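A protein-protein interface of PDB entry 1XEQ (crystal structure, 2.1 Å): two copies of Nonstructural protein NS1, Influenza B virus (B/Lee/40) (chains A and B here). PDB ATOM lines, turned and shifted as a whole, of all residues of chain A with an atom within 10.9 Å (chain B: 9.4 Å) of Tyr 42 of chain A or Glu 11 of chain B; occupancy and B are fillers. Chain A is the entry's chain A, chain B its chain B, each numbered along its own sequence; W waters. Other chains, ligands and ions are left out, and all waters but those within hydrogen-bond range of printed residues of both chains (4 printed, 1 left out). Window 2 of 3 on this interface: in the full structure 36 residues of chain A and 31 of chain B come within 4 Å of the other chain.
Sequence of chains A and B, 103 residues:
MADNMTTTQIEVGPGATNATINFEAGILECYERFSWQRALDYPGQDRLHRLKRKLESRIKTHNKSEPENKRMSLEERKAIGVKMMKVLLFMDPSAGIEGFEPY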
ATOM      1  N   TYR A  31      30.641  18.161  -9.128  1.00  0.00           N
ATOM      2  CA  TYR A  31      30.363  18.276  -7.641  1.00  0.00           C
ATOM      3  C   TYR A  31      31.228  19.328  -7.086  1.00  0.00           C
ATOM      4  O   TYR A  31      30.789  20.169  -6.330  1.00  0.00           O
ATOM      5  CB  TYR A  31      30.639  16.968  -6.940  1.00  0.00           C
ATOM      6  CG  TYR A  31      29.493  15.996  -6.885  1.00  0.00           C
ATOM      7  CD1 TYR A  31      29.259  15.092  -7.877  1.00  0.00           C
ATOM      8  CD2 TYR A  31      28.695  15.932  -5.768  1.00  0.00           C
ATOM      9  CE1 TYR A  31      28.217  14.192  -7.805  1.00  0.00           C
ATOM     10  CE2 TYR A  31      27.632  15.073  -5.718  1.00  0.00           C
ATOM     11  CZ  TYR A  31      27.426  14.162  -6.677  1.00  0.00           C
ATOM     12  OH  TYR A  31      26.326  13.292  -6.568  1.00  0.00           O
ATOM     13  N   PHE A  34      30.111  22.763  -8.156  1.00  0.00           N
ATOM     14  CA  PHE A  34      28.881  23.148  -7.511  1.00  0.00           C
ATOM     15  C   PHE A  34      29.232  23.514  -6.024  1.00  0.00           C
ATOM     16  O   PHE A  34      28.701  24.475  -5.468  1.00  0.00           O
ATOM     17  CB  PHE A  34      27.934  21.970  -7.642  1.00  0.00           C
ATOM     18  CG  PHE A  34      26.546  22.236  -7.293  1.00  0.00           C
ATOM     19  CD1 PHE A  34      25.782  23.135  -8.006  1.00  0.00           C
ATOM     20  CD2 PHE A  34      25.954  21.541  -6.242  1.00  0.00           C
ATOM     21  CE1 PHE A  34      24.442  23.300  -7.697  1.00  0.00           C
ATOM     22  CE2 PHE A  34      24.660  21.707  -5.935  1.00  0.00           C
ATOM     23  CZ  PHE A  34      23.888  22.583  -6.633  1.00  0.00           C
ATOM     24  N   SER A  35      30.196  22.822  -5.442  1.00  0.00           N
ATOM     25  CA  SER A  35      30.493  23.002  -3.999  1.00  0.00           C
ATOM     26  C   SER A  35      31.188  24.350  -3.814  1.00  0.00           C
ATOM     27  O   SER A  35      30.932  25.089  -2.873  1.00  0.00           O
ATOM     28  CB  SER A  35      31.390  21.874  -3.458  1.00  0.00           C
ATOM     29  OG  SER A  35      31.505  21.999  -2.028  1.00  0.00           O
ATOM     30  N   TRP A  36      32.060  24.676  -4.764  1.00  0.00           N
ATOM     31  CA  TRP A  36      32.706  25.964  -4.847  1.00  0.00           C
ATOM     32  C   TRP A  36      31.673  27.098  -4.857  1.00  0.00           C
ATOM     33  O   TRP A  36      31.855  28.125  -4.302  1.00  0.00           O
ATOM     34  CB  TRP A  36      33.477  25.919  -6.182  1.00  0.00           C
ATOM     35  CG  TRP A  36      33.962  27.111  -6.805  1.00  0.00           C
ATOM     36  CD1 TRP A  36      34.556  28.158  -6.192  1.00  0.00           C
ATOM     37  CD2 TRP A  36      34.018  27.393  -8.262  1.00  0.00           C
ATOM     38  NE1 TRP A  36      34.936  29.076  -7.144  1.00  0.00           N
ATOM     39  CE2 TRP A  36      34.607  28.623  -8.411  1.00  0.00           C
ATOM     40  CE3 TRP A  36      33.560  26.731  -9.409  1.00  0.00           C
ATOM     41  CZ2 TRP A  36      34.838  29.201  -9.674  1.00  0.00           C
ATOM     42  CZ3 TRP A  36      33.822  27.258 -10.693  1.00  0.00           C
ATOM     43  CH2 TRP A  36      34.449  28.491 -10.810  1.00  0.00           C
ATOM     44  N   GLN A  37      30.575  26.892  -5.523  1.00  0.00           N
ATOM     45  CA  GLN A  37      29.541  27.926  -5.547  1.00  0.00           C
ATOM     46  C   GLN A  37      28.609  27.910  -4.292  1.00  0.00           C
ATOM     47  O   GLN A  37      27.598  28.609  -4.298  1.00  0.00           O
ATOM     48  CB  GLN A  37      28.726  27.734  -6.817  1.00  0.00           C
ATOM     49  CG  GLN A  37      29.462  28.147  -8.123  1.00  0.00           C
ATOM     50  CD  GLN A  37      30.189  29.474  -7.998  1.00  0.00           C
ATOM     51  OE1 GLN A  37      31.431  29.504  -7.927  1.00  0.00           O
ATOM     52  NE2 GLN A  37      29.440  30.560  -7.919  1.00  0.00           N
ATOM     53  N   ARG A  38      28.936  27.134  -3.254  1.00  0.00           N
ATOM     54  CA  ARG A  38      28.182  27.084  -1.990  1.00  0.00           C
ATOM     55  C   ARG A  38      26.713  26.591  -2.187  1.00  0.00           C
ATOM     56  O   ARG A  38      25.791  27.001  -1.474  1.00  0.00           O
ATOM     57  CB  ARG A  38      28.182  28.442  -1.258  1.00  0.00           C
ATOM     58  CG  ARG A  38      29.491  29.007  -0.699  1.00  0.00           C
ATOM     59  CD  ARG A  38      29.211  30.169   0.247  1.00  0.00           C
ATOM     60  NE  ARG A  38      30.434  30.875   0.680  1.00  0.00           N
ATOM     61  CZ  ARG A  38      31.245  30.470   1.623  1.00  0.00           C
ATOM     62  NH1 ARG A  38      31.007  29.345   2.256  1.00  0.00           N
ATOM     63  NH2 ARG A  38      32.344  31.197   1.903  1.00  0.00           N
ATOM     64  N   ALA A  39      26.515  25.706  -3.152  1.00  0.00           N
ATOM     65  CA  ALA A  39      25.255  25.084  -3.388  1.00  0.00           C
ATOM     66  C   ALA A  39      25.216  23.634  -2.954  1.00  0.00           C
ATOM     67  O   ALA A  39      24.166  23.054  -2.954  1.00  0.00           O
ATOM     68  CB  ALA A  39      24.919  25.184  -4.880  1.00  0.00           C
ATOM     69  N   LEU A  40      26.366  23.014  -2.690  1.00  0.00           N
ATOM     70  CA  LEU A  40      26.403  21.613  -2.298  1.00  0.00           C
ATOM     71  C   LEU A  40      26.251  21.496  -0.775  1.00  0.00           C
ATOM     72  O   LEU A  40      27.046  22.057  -0.039  1.00  0.00           O
ATOM     73  CB  LEU A  40      27.699  20.981  -2.723  1.00  0.00           C
ATOM     74  CG  LEU A  40      27.785  19.448  -2.571  1.00  0.00           C
ATOM     75  CD1 LEU A  40      26.807  18.671  -3.499  1.00  0.00           C
ATOM     76  CD2 LEU A  40      29.187  19.023  -2.892  1.00  0.00           C
ATOM     77  N   ASP A  41      25.265  20.740  -0.336  1.00  0.00           N
ATOM     78  CA  ASP A  41      24.930  20.651   1.080  1.00  0.00           C
ATOM     79  C   ASP A  41      25.868  19.740   1.794  1.00  0.00           C
ATOM     80  O   ASP A  41      26.772  19.146   1.214  1.00  0.00           O
ATOM     81  CB  ASP A  41      23.446  20.308   1.319  1.00  0.00           C
ATOM     82  CG  ASP A  41      23.053  18.920   0.886  1.00  0.00           C
ATOM     83  OD1 ASP A  41      23.907  18.054   0.586  1.00  0.00           O
ATOM     84  OD2 ASP A  41      21.861  18.595   0.900  1.00  0.00           O
ATOM     85  N   TYR A  42      25.734  19.640   3.087  1.00  0.00           N
ATOM     86  CA  TYR A  42      26.807  18.914   3.820  1.00  0.00           C
ATOM     87  C   TYR A  42      26.878  17.428   3.505  1.00  0.00           C
ATOM     88  O   TYR A  42      27.939  16.915   3.271  1.00  0.00           O
ATOM     89  CB  TYR A  42      26.715  19.178   5.327  1.00  0.00           C
ATOM     90  CG  TYR A  42      26.761  20.638   5.606  1.00  0.00           C
ATOM     91  CD1 TYR A  42      25.823  21.246   6.403  1.00  0.00           C
ATOM     92  CD2 TYR A  42      27.773  21.424   5.080  1.00  0.00           C
ATOM     93  CE1 TYR A  42      25.834  22.580   6.624  1.00  0.00           C
ATOM     94  CE2 TYR A  42      27.807  22.798   5.300  1.00  0.00           C
ATOM     95  CZ  TYR A  42      26.844  23.359   6.080  1.00  0.00           C
ATOM     96  OH  TYR A  42      26.876  24.704   6.270  1.00  0.00           O
ATOM     97  N   PRO A  43      25.789  16.703   3.454  1.00  0.00           N
ATOM     98  CA  PRO A  43      25.888  15.306   3.038  1.00  0.00           C
ATOM     99  C   PRO A  43      26.384  15.214   1.541  1.00  0.00           C
ATOM    100  O   PRO A  43      27.089  14.282   1.134  1.00  0.00           O
ATOM    101  CB  PRO A  43      24.478  14.811   3.194  1.00  0.00           C
ATOM    102  CG  PRO A  43      23.863  15.699   4.094  1.00  0.00           C
ATOM    103  CD  PRO A  43      24.416  17.063   3.800  1.00  0.00           C
ATOM    104  N   GLY A  44      26.082  16.234   0.761  1.00  0.00           N
ATOM    105  CA  GLY A  44      26.609  16.264  -0.630  1.00  0.00           C
ATOM    106  C   GLY A  44      28.098  16.385  -0.679  1.00  0.00           C
ATOM    107  O   GLY A  44      28.730  15.762  -1.493  1.00  0.00           O
ATOM    108  N   GLN A  45      28.643  17.240   0.167  1.00  0.00           N
ATOM    109  CA  GLN A  45      30.101  17.378   0.259  1.00  0.00           C
ATOM    110  C   GLN A  45      30.754  16.064   0.829  1.00  0.00           C
ATOM    111  O   GLN A  45      31.813  15.678   0.356  1.00  0.00           O
ATOM    112  CB  GLN A  45      30.498  18.608   1.094  1.00  0.00           C
ATOM    113  CG  GLN A  45      29.987  19.975   0.566  1.00  0.00           C
ATOM    114  CD  GLN A  45      30.306  21.115   1.479  1.00  0.00           C
ATOM    115  OE1 GLN A  45      31.440  21.203   1.945  1.00  0.00           O
ATOM    116  NE2 GLN A  45      29.325  22.019   1.729  1.00  0.00           N
ATOM    117  N   ASP A  46      30.110  15.368   1.764  1.00  0.00           N
ATOM    118  CA  ASP A  46      30.606  14.010   2.215  1.00  0.00           C
ATOM    119  C   ASP A  46      30.658  13.122   0.977  1.00  0.00           C
ATOM    120  O   ASP A  46      31.649  12.426   0.700  1.00  0.00           O
ATOM    121  CB  ASP A  46      29.640  13.356   3.222  1.00  0.00           C
ATOM    122  CG  ASP A  46      29.754  13.982   4.651  1.00  0.00           C
ATOM    123  OD1 ASP A  46      30.747  14.721   4.877  1.00  0.00           O
ATOM    124  OD2 ASP A  46      28.929  13.736   5.564  1.00  0.00           O
ATOM    125  N   ARG A  47      29.565  13.160   0.222  1.00  0.00           N
ATOM    126  CA  ARG A  47      29.475  12.338  -1.028  1.00  0.00           C
ATOM    127  C   ARG A  47      30.635  12.696  -1.969  1.00  0.00           C
ATOM    128  O   ARG A  47      31.354  11.821  -2.467  1.00  0.00           O
ATOM    129  CB  ARG A  47      28.119  12.530  -1.716  1.00  0.00           C
ATOM    130  CG  ARG A  47      27.845  11.571  -2.853  1.00  0.00           C
ATOM    131  CD  ARG A  47      26.500  11.713  -3.501  1.00  0.00           C
ATOM    132  NE  ARG A  47      26.398  10.773  -4.631  1.00  0.00           N
ATOM    133  CZ  ARG A  47      25.889   9.538  -4.537  1.00  0.00           C
ATOM    134  NH1 ARG A  47      25.397   9.028  -3.397  1.00  0.00           N
ATOM    135  NH2 ARG A  47      25.911   8.768  -5.578  1.00  0.00           N
ATOM    136  N   LEU A  48      30.890  13.988  -2.163  1.00  0.00           N
ATOM    137  CA  LEU A  48      32.009  14.410  -3.002  1.00  0.00           C
ATOM    138  C   LEU A  48      33.335  13.827  -2.454  1.00  0.00           C
ATOM    139  O   LEU A  48      34.137  13.320  -3.178  1.00  0.00           O
ATOM    140  CB  LEU A  48      32.055  15.917  -3.037  1.00  0.00           C
ATOM    141  CG  LEU A  48      32.999  16.704  -3.920  1.00  0.00           C
ATOM    142  CD1 LEU A  48      32.799  18.241  -3.702  1.00  0.00           C
ATOM    143  CD2 LEU A  48      34.439  16.372  -3.616  1.00  0.00           C
ATOM    144  N   HIS A  49      33.556  13.911  -1.151  1.00  0.00           N
ATOM    145  CA  HIS A  49      34.791  13.343  -0.591  1.00  0.00           C
ATOM    146  C   HIS A  49      34.867  11.846  -0.819  1.00  0.00           C
ATOM    147  O   HIS A  49      35.876  11.361  -1.204  1.00  0.00           O
ATOM    148  CB  HIS A  49      34.909  13.717   0.889  1.00  0.00           C
ATOM    149  CG  HIS A  49      34.859  15.192   1.110  1.00  0.00           C
ATOM    150  ND1 HIS A  49      35.637  16.079   0.374  1.00  0.00           N
ATOM    151  CD2 HIS A  49      34.098  15.947   1.943  1.00  0.00           C
ATOM    152  CE1 HIS A  49      35.318  17.315   0.726  1.00  0.00           C
ATOM    153  NE2 HIS A  49      34.403  17.262   1.683  1.00  0.00           N
ATOM    154  N   ARG A  50      33.791  11.098  -0.669  1.00  0.00           N
ATOM    155  CA  ARG A  50      33.881   9.657  -0.925  1.00  0.00           C
ATOM    156  C   ARG A  50      34.226   9.390  -2.381  1.00  0.00           C
ATOM    157  O   ARG A  50      35.100   8.589  -2.747  1.00  0.00           O
ATOM    158  CB  ARG A  50      32.588   8.918  -0.647  1.00  0.00           C
ATOM    159  CG  ARG A  50      32.301   8.454   0.818  1.00  0.00           C
ATOM    160  CD  ARG A  50      30.854   7.795   0.834  1.00  0.00           C
ATOM    161  NE  ARG A  50      30.043   8.831   1.307  1.00  0.00           N
ATOM    162  CZ  ARG A  50      28.884   9.207   0.957  1.00  0.00           C
ATOM    163  NH1 ARG A  50      28.152   8.660   0.007  1.00  0.00           N
ATOM    164  NH2 ARG A  50      28.440  10.188   1.654  1.00  0.00           N
ATOM    165  N   GLN B   9      35.100  21.554   5.029  1.00  0.00           N
ATOM    166  CA  GLN B   9      33.798  21.710   4.373  1.00  0.00           C
ATOM    167  C   GLN B   9      33.517  23.177   4.088  1.00  0.00           C
ATOM    168  O   GLN B   9      34.016  24.090   4.786  1.00  0.00           O
ATOM    169  CB  GLN B   9      32.651  21.154   5.248  1.00  0.00           C
ATOM    170  CG  GLN B   9      32.721  19.643   5.696  1.00  0.00           C
ATOM    171  CD  GLN B   9      32.158  18.617   4.709  1.00  0.00           C
ATOM    172  OE1 GLN B   9      32.902  18.161   3.846  1.00  0.00           O
ATOM    173  NE2 GLN B   9      30.883  18.207   4.870  1.00  0.00           N
ATOM    174  N   ILE B  10      32.638  23.404   3.135  1.00  0.00           N
ATOM    175  CA  ILE B  10      32.157  24.746   2.824  1.00  0.00           C
ATOM    176  C   ILE B  10      30.818  25.060   3.487  1.00  0.00           C
ATOM    177  O   ILE B  10      29.843  24.328   3.372  1.00  0.00           O
ATOM    178  CB  ILE B  10      32.144  24.877   1.272  1.00  0.00           C
ATOM    179  CG1 ILE B  10      33.597  24.681   0.800  1.00  0.00           C
ATOM    180  CG2 ILE B  10      31.569  26.189   0.823  1.00  0.00           C
ATOM    181  CD1 ILE B  10      33.802  24.361  -0.611  1.00  0.00           C
ATOM    182  N   GLU B  11      30.768  26.176   4.199  1.00  0.00           N
ATOM    183  CA  GLU B  11      29.520  26.611   4.791  1.00  0.00           C
ATOM    184  C   GLU B  11      28.513  27.032   3.720  1.00  0.00           C
ATOM    185  O   GLU B  11      28.850  27.799   2.811  1.00  0.00           O
ATOM    186  CB  GLU B  11      29.798  27.802   5.721  1.00  0.00           C
ATOM    187  CG  GLU B  11      28.481  28.338   6.291  1.00  0.00           C
ATOM    188  CD  GLU B  11      28.646  28.945   7.692  1.00  0.00           C
ATOM    189  OE1 GLU B  11      27.664  29.557   8.214  1.00  0.00           O
ATOM    190  OE2 GLU B  11      29.730  28.790   8.304  1.00  0.00           O
ATOM    191  N   VAL B  12      27.275  26.573   3.849  1.00  0.00           N
ATOM    192  CA  VAL B  12      26.207  26.878   2.919  1.00  0.00           C
ATOM    193  C   VAL B  12      24.908  27.240   3.644  1.00  0.00           C
ATOM    194  O   VAL B  12      24.733  26.894   4.824  1.00  0.00           O
ATOM    195  CB  VAL B  12      25.947  25.720   1.950  1.00  0.00           C
ATOM    196  CG1 VAL B  12      27.192  25.332   1.216  1.00  0.00           C
ATOM    197  CG2 VAL B  12      25.343  24.470   2.705  1.00  0.00           C
ATOM    198  N   GLY B  13      24.049  27.960   2.910  1.00  0.00           N
ATOM    199  CA  GLY B  13      22.669  28.312   3.265  1.00  0.00           C
ATOM    200  C   GLY B  13      21.673  27.193   3.133  1.00  0.00           C
ATOM    201  O   GLY B  13      21.935  26.166   2.490  1.00  0.00           O
ATOM    202  N   PRO B  14      20.483  27.400   3.735  1.00  0.00           N
ATOM    203  CA  PRO B  14      19.380  26.439   3.640  1.00  0.00           C
ATOM    204  C   PRO B  14      18.996  26.145   2.162  1.00  0.00           C
ATOM    205  O   PRO B  14      18.490  25.065   1.898  1.00  0.00           O
ATOM    206  CB  PRO B  14      18.220  27.105   4.420  1.00  0.00           C
ATOM    207  CG  PRO B  14      18.615  28.586   4.509  1.00  0.00           C
ATOM    208  CD  PRO B  14      20.130  28.590   4.540  1.00  0.00           C
ATOM    209  N   GLY B  15      19.294  27.050   1.226  1.00  0.00           N
ATOM    210  CA  GLY B  15      18.983  26.800  -0.180  1.00  0.00           C
ATOM    211  C   GLY B  15      19.687  25.589  -0.762  1.00  0.00           C
ATOM    212  O   GLY B  15      19.258  25.039  -1.780  1.00  0.00           O
ATOM    213  N   ALA B  16      20.751  25.117  -0.105  1.00  0.00           N
ATOM    214  CA  ALA B  16      21.558  24.038  -0.648  1.00  0.00           C
ATOM    215  C   ALA B  16      20.910  22.687  -0.601  1.00  0.00           C
ATOM    216  O   ALA B  16      21.318  21.780  -1.340  1.00  0.00           O
ATOM    217  CB  ALA B  16      22.876  24.015   0.025  1.00  0.00           C
ATOM    218  N   THR B  17      19.928  22.518   0.301  1.00  0.00           N
ATOM    219  CA  THR B  17      19.184  21.250   0.357  1.00  0.00           C
ATOM    220  C   THR B  17      18.492  20.972  -0.944  1.00  0.00           C
ATOM    221  O   THR B  17      18.744  19.938  -1.582  1.00  0.00           O
ATOM    222  CB  THR B  17      18.140  21.271   1.493  1.00  0.00           C
ATOM    223  OG1 THR B  17      18.885  21.318   2.695  1.00  0.00           O
ATOM    224  CG2 THR B  17      17.383  19.887   1.615  1.00  0.00           C
ATOM    225  N   THR B  20      20.884  20.733  -3.970  1.00  0.00           N
ATOM    226  CA  THR B  20      21.669  19.519  -4.050  1.00  0.00           C
ATOM    227  C   THR B  20      20.836  18.347  -4.547  1.00  0.00           C
ATOM    228  O   THR B  20      21.271  17.552  -5.363  1.00  0.00           O
ATOM    229  CB  THR B  20      22.329  19.192  -2.723  1.00  0.00           C
ATOM    230  OG1 THR B  20      23.346  20.124  -2.437  1.00  0.00           O
ATOM    231  CG2 THR B  20      23.052  17.859  -2.753  1.00  0.00           C
ATOM    232  N   GLU B  24      21.793  16.653  -7.946  1.00  0.00           N
ATOM    233  CA  GLU B  24      21.984  15.237  -8.080  1.00  0.00           C
ATOM    234  C   GLU B  24      21.006  14.572  -9.020  1.00  0.00           C
ATOM    235  O   GLU B  24      21.308  13.535  -9.600  1.00  0.00           O
ATOM    236  CB  GLU B  24      22.027  14.527  -6.711  1.00  0.00           C
ATOM    237  CG  GLU B  24      23.223  14.949  -5.934  1.00  0.00           C
ATOM    238  CD  GLU B  24      23.259  14.423  -4.487  1.00  0.00           C
ATOM    239  OE1 GLU B  24      22.272  13.970  -3.983  1.00  0.00           O
ATOM    240  OE2 GLU B  24      24.307  14.508  -3.873  1.00  0.00           O
ATOM    241  N   ARG B  58      14.735  11.008  -0.783  1.00  0.00           N
ATOM    242  CA  ARG B  58      14.996  12.389  -0.386  1.00  0.00           C
ATOM    243  C   ARG B  58      13.976  13.350  -0.946  1.00  0.00           C
ATOM    244  O   ARG B  58      13.575  14.304  -0.270  1.00  0.00           O
ATOM    245  CB  ARG B  58      16.371  12.807  -0.774  1.00  0.00           C
ATOM    246  CG  ARG B  58      17.433  12.062  -0.083  1.00  0.00           C
ATOM    247  CD  ARG B  58      18.807  12.618  -0.389  1.00  0.00           C
ATOM    248  NE  ARG B  58      19.385  11.939  -1.527  1.00  0.00           N
ATOM    249  CZ  ARG B  58      20.556  12.217  -2.050  1.00  0.00           C
ATOM    250  NH1 ARG B  58      21.292  13.161  -1.529  1.00  0.00           N
ATOM    251  NH2 ARG B  58      20.990  11.531  -3.084  1.00  0.00           N
HETATM  252  O   HOH W   1      19.990  17.596  -0.296  1.00  0.00           O
HETATM  253  O   HOH W   2      22.581  15.453   0.104  1.00  0.00           O
HETATM  254  O   HOH W   3      20.554  19.627   3.097  1.00  0.00           O
HETATM  255  O   HOH W   4      24.769  28.866   0.349  1.00  0.00           O
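Hydrophobic or aromatic side chains of chain B that line the printed part of chain A: Ile 10, Val 12 and Ala 16. Hydrophobic or aromatic side chains of chain A that line the printed part of chain B: Tyr 31, Leu 40, Tyr 42 and His 49. Among the printed residues, 22 pairs touch across the chains.
No position is printed for both chains. Of the 22 pairs that touch across the chains among the printed residues, none has its exchanged pair printed and touching as well.
Of the printed residues of chain B, Tyr 42 of chain A touches Gln 9, Ile 10, Glu 11 and Val 12. Of chain A, only Arg 38 (2.7 Å) and Tyr 42 (3.6 Å) come within 4 Å of Glu 11 of chain B. Asp 41 of chain A touches just these residues of chain B: Ala 16, Thr 17 and Thr 20. No residue of chain B comes within 4 Å of Pro 43 of chain A. No residue of chain B comes within 4 Å of Gly 44 of chain A. Gln 45 of chain A touches three residues of chain B. Of the printed residues of chain A, Gln 9 of chain B touches Tyr 42, Gln 45, Asp 46 and His 49. Of chain A, only Ser 35, Arg 38, Tyr 42 and Gln 45 come within 4 Å of Ile 10 of chain B. No residue of chain A comes within 4 Å of Gly 13 of chain B. Printed residues of chain A within 4 Å of Glu 24 of chain B: Tyr 31 (3.6 Å) and Arg 47 (3.6 Å). Printed residues of chain A within 4 Å of Thr 20 of chain B: Ala 39, Leu 40 and Asp 41. Arg 58 of chain B touches none of the printed residues of chain A. The nearest residue of chain B that does not touch Tyr 42 of chain A is Gly 13 of chain B (5.5 Å). The nearest printed residue of chain B that does not touch Ser 35 of chain A is Val 12 of chain B (5.5 Å).
Water W3 lies within hydrogen-bond range of the side-chain hydroxyl (OG1) of Thr 17 of chain B (2.4 Å) and the side-chain carboxylate (OD2) of Asp 41 of chain A (2.8 Å). Water W1 bridges the side-chain carboxylate (OD2) of Asp 41 of chain A (2.4 Å) and the backbone carbonyl oxygen (O) of Thr 17 of chain B (2.9 Å). Water W4 lies within hydrogen-bond range of O of Arg 38 of chain A and N of Gly 13 of chain B. Water W2 bridges OD1 of Asp 41 of chain A (3.0 Å) and NH1 of Arg 58 of chain B (3.1 Å).
The side-chain carboxylate (OD1) of Asp 41 of chain A is in hydrogen-bond range of the backbone NH (N) of Gly 44 of chain A, at 2.8 Å. The guanidinium group (NE) of Arg 47 of chain A sits at hydrogen-bond distance from the side-chain hydroxyl (OH) of Tyr 31 of chain A. OE1 of Glu 24 of chain B is in salt-bridge range of NH1 of Arg 58 of chain B. The backbone carbonyl oxygen (O) of Phe 34 of chain A is in hydrogen-bond range of the backbone NH (N) of Ala 39 of chain A. O of Leu 40 of chain A lies within hydrogen-bond range of NE2 of Gln 45 of chain A (2.9 Å). The backbone carbonyl oxygen (O) of Ala 16 of chain B is in hydrogen-bond range of the side-chain hydroxyl (OG1) of Thr 20 of chain B (2.8 Å).
Among the printed residues, pairs that only touch across the chains: Tyr 42 of chain A with Ile 10 of chain B, Ala 39 of chain A with Ala 16 of chain B, Leu 40 of chain A with Thr 20 of chain B, Gln 45 of chain A with Gln 9 of chain B, Arg 38 of chain A with Val 12 of chain B, Leu 40 of chain A with Val 12 of chain B, Arg 38 of chain A with Ile 10 of chain B, Arg 47 of chain A with Glu 24 of chain B, Tyr 31 of chain A with Glu 24 of chain B, Tyr 42 of chain A with Glu 11 of chain B, Ser 35 of chain A with Ile 10 of chain B, Tyr 42 of chain A with Gln 9 of chain B, Asp 41 of chain A with Ala 16 of chain B, Asp 41 of chain A with Thr 17 of chain B and Gln 45 of chain A with Val 12 of chain B.
The side-chain amide oxygen of Gln 45 of chain A lies within hydrogen-bond range of the backbone NH of Ile 10 of chain B (2.8 Å). N of Asp 41 of chain A is in hydrogen-bond range of OG1 of Thr 20 of chain B (2.9 Å). O of Ala 39 of chain A lies within hydrogen-bond range of OG1 of Thr 20 of chain B, at 3.1 Å. A ring nitrogen (NE2) of His 49 of chain A sits at hydrogen-bond distance from the side-chain amide oxygen (OE1) of Gln 9 of chain B, 2.8 Å away. The side-chain hydroxyl (OH) of Tyr 42 of chain A sits at hydrogen-bond distance from the backbone NH (N) of Val 12 of chain B, 3.1 Å away. NH1 of Arg 38 of chain A lies within hydrogen-bond range of O of Glu 11 of chain B. OD1 of Asp 46 of chain A is in hydrogen-bond range of NE2 of Gln 9 of chain B, 3.5 Å away.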
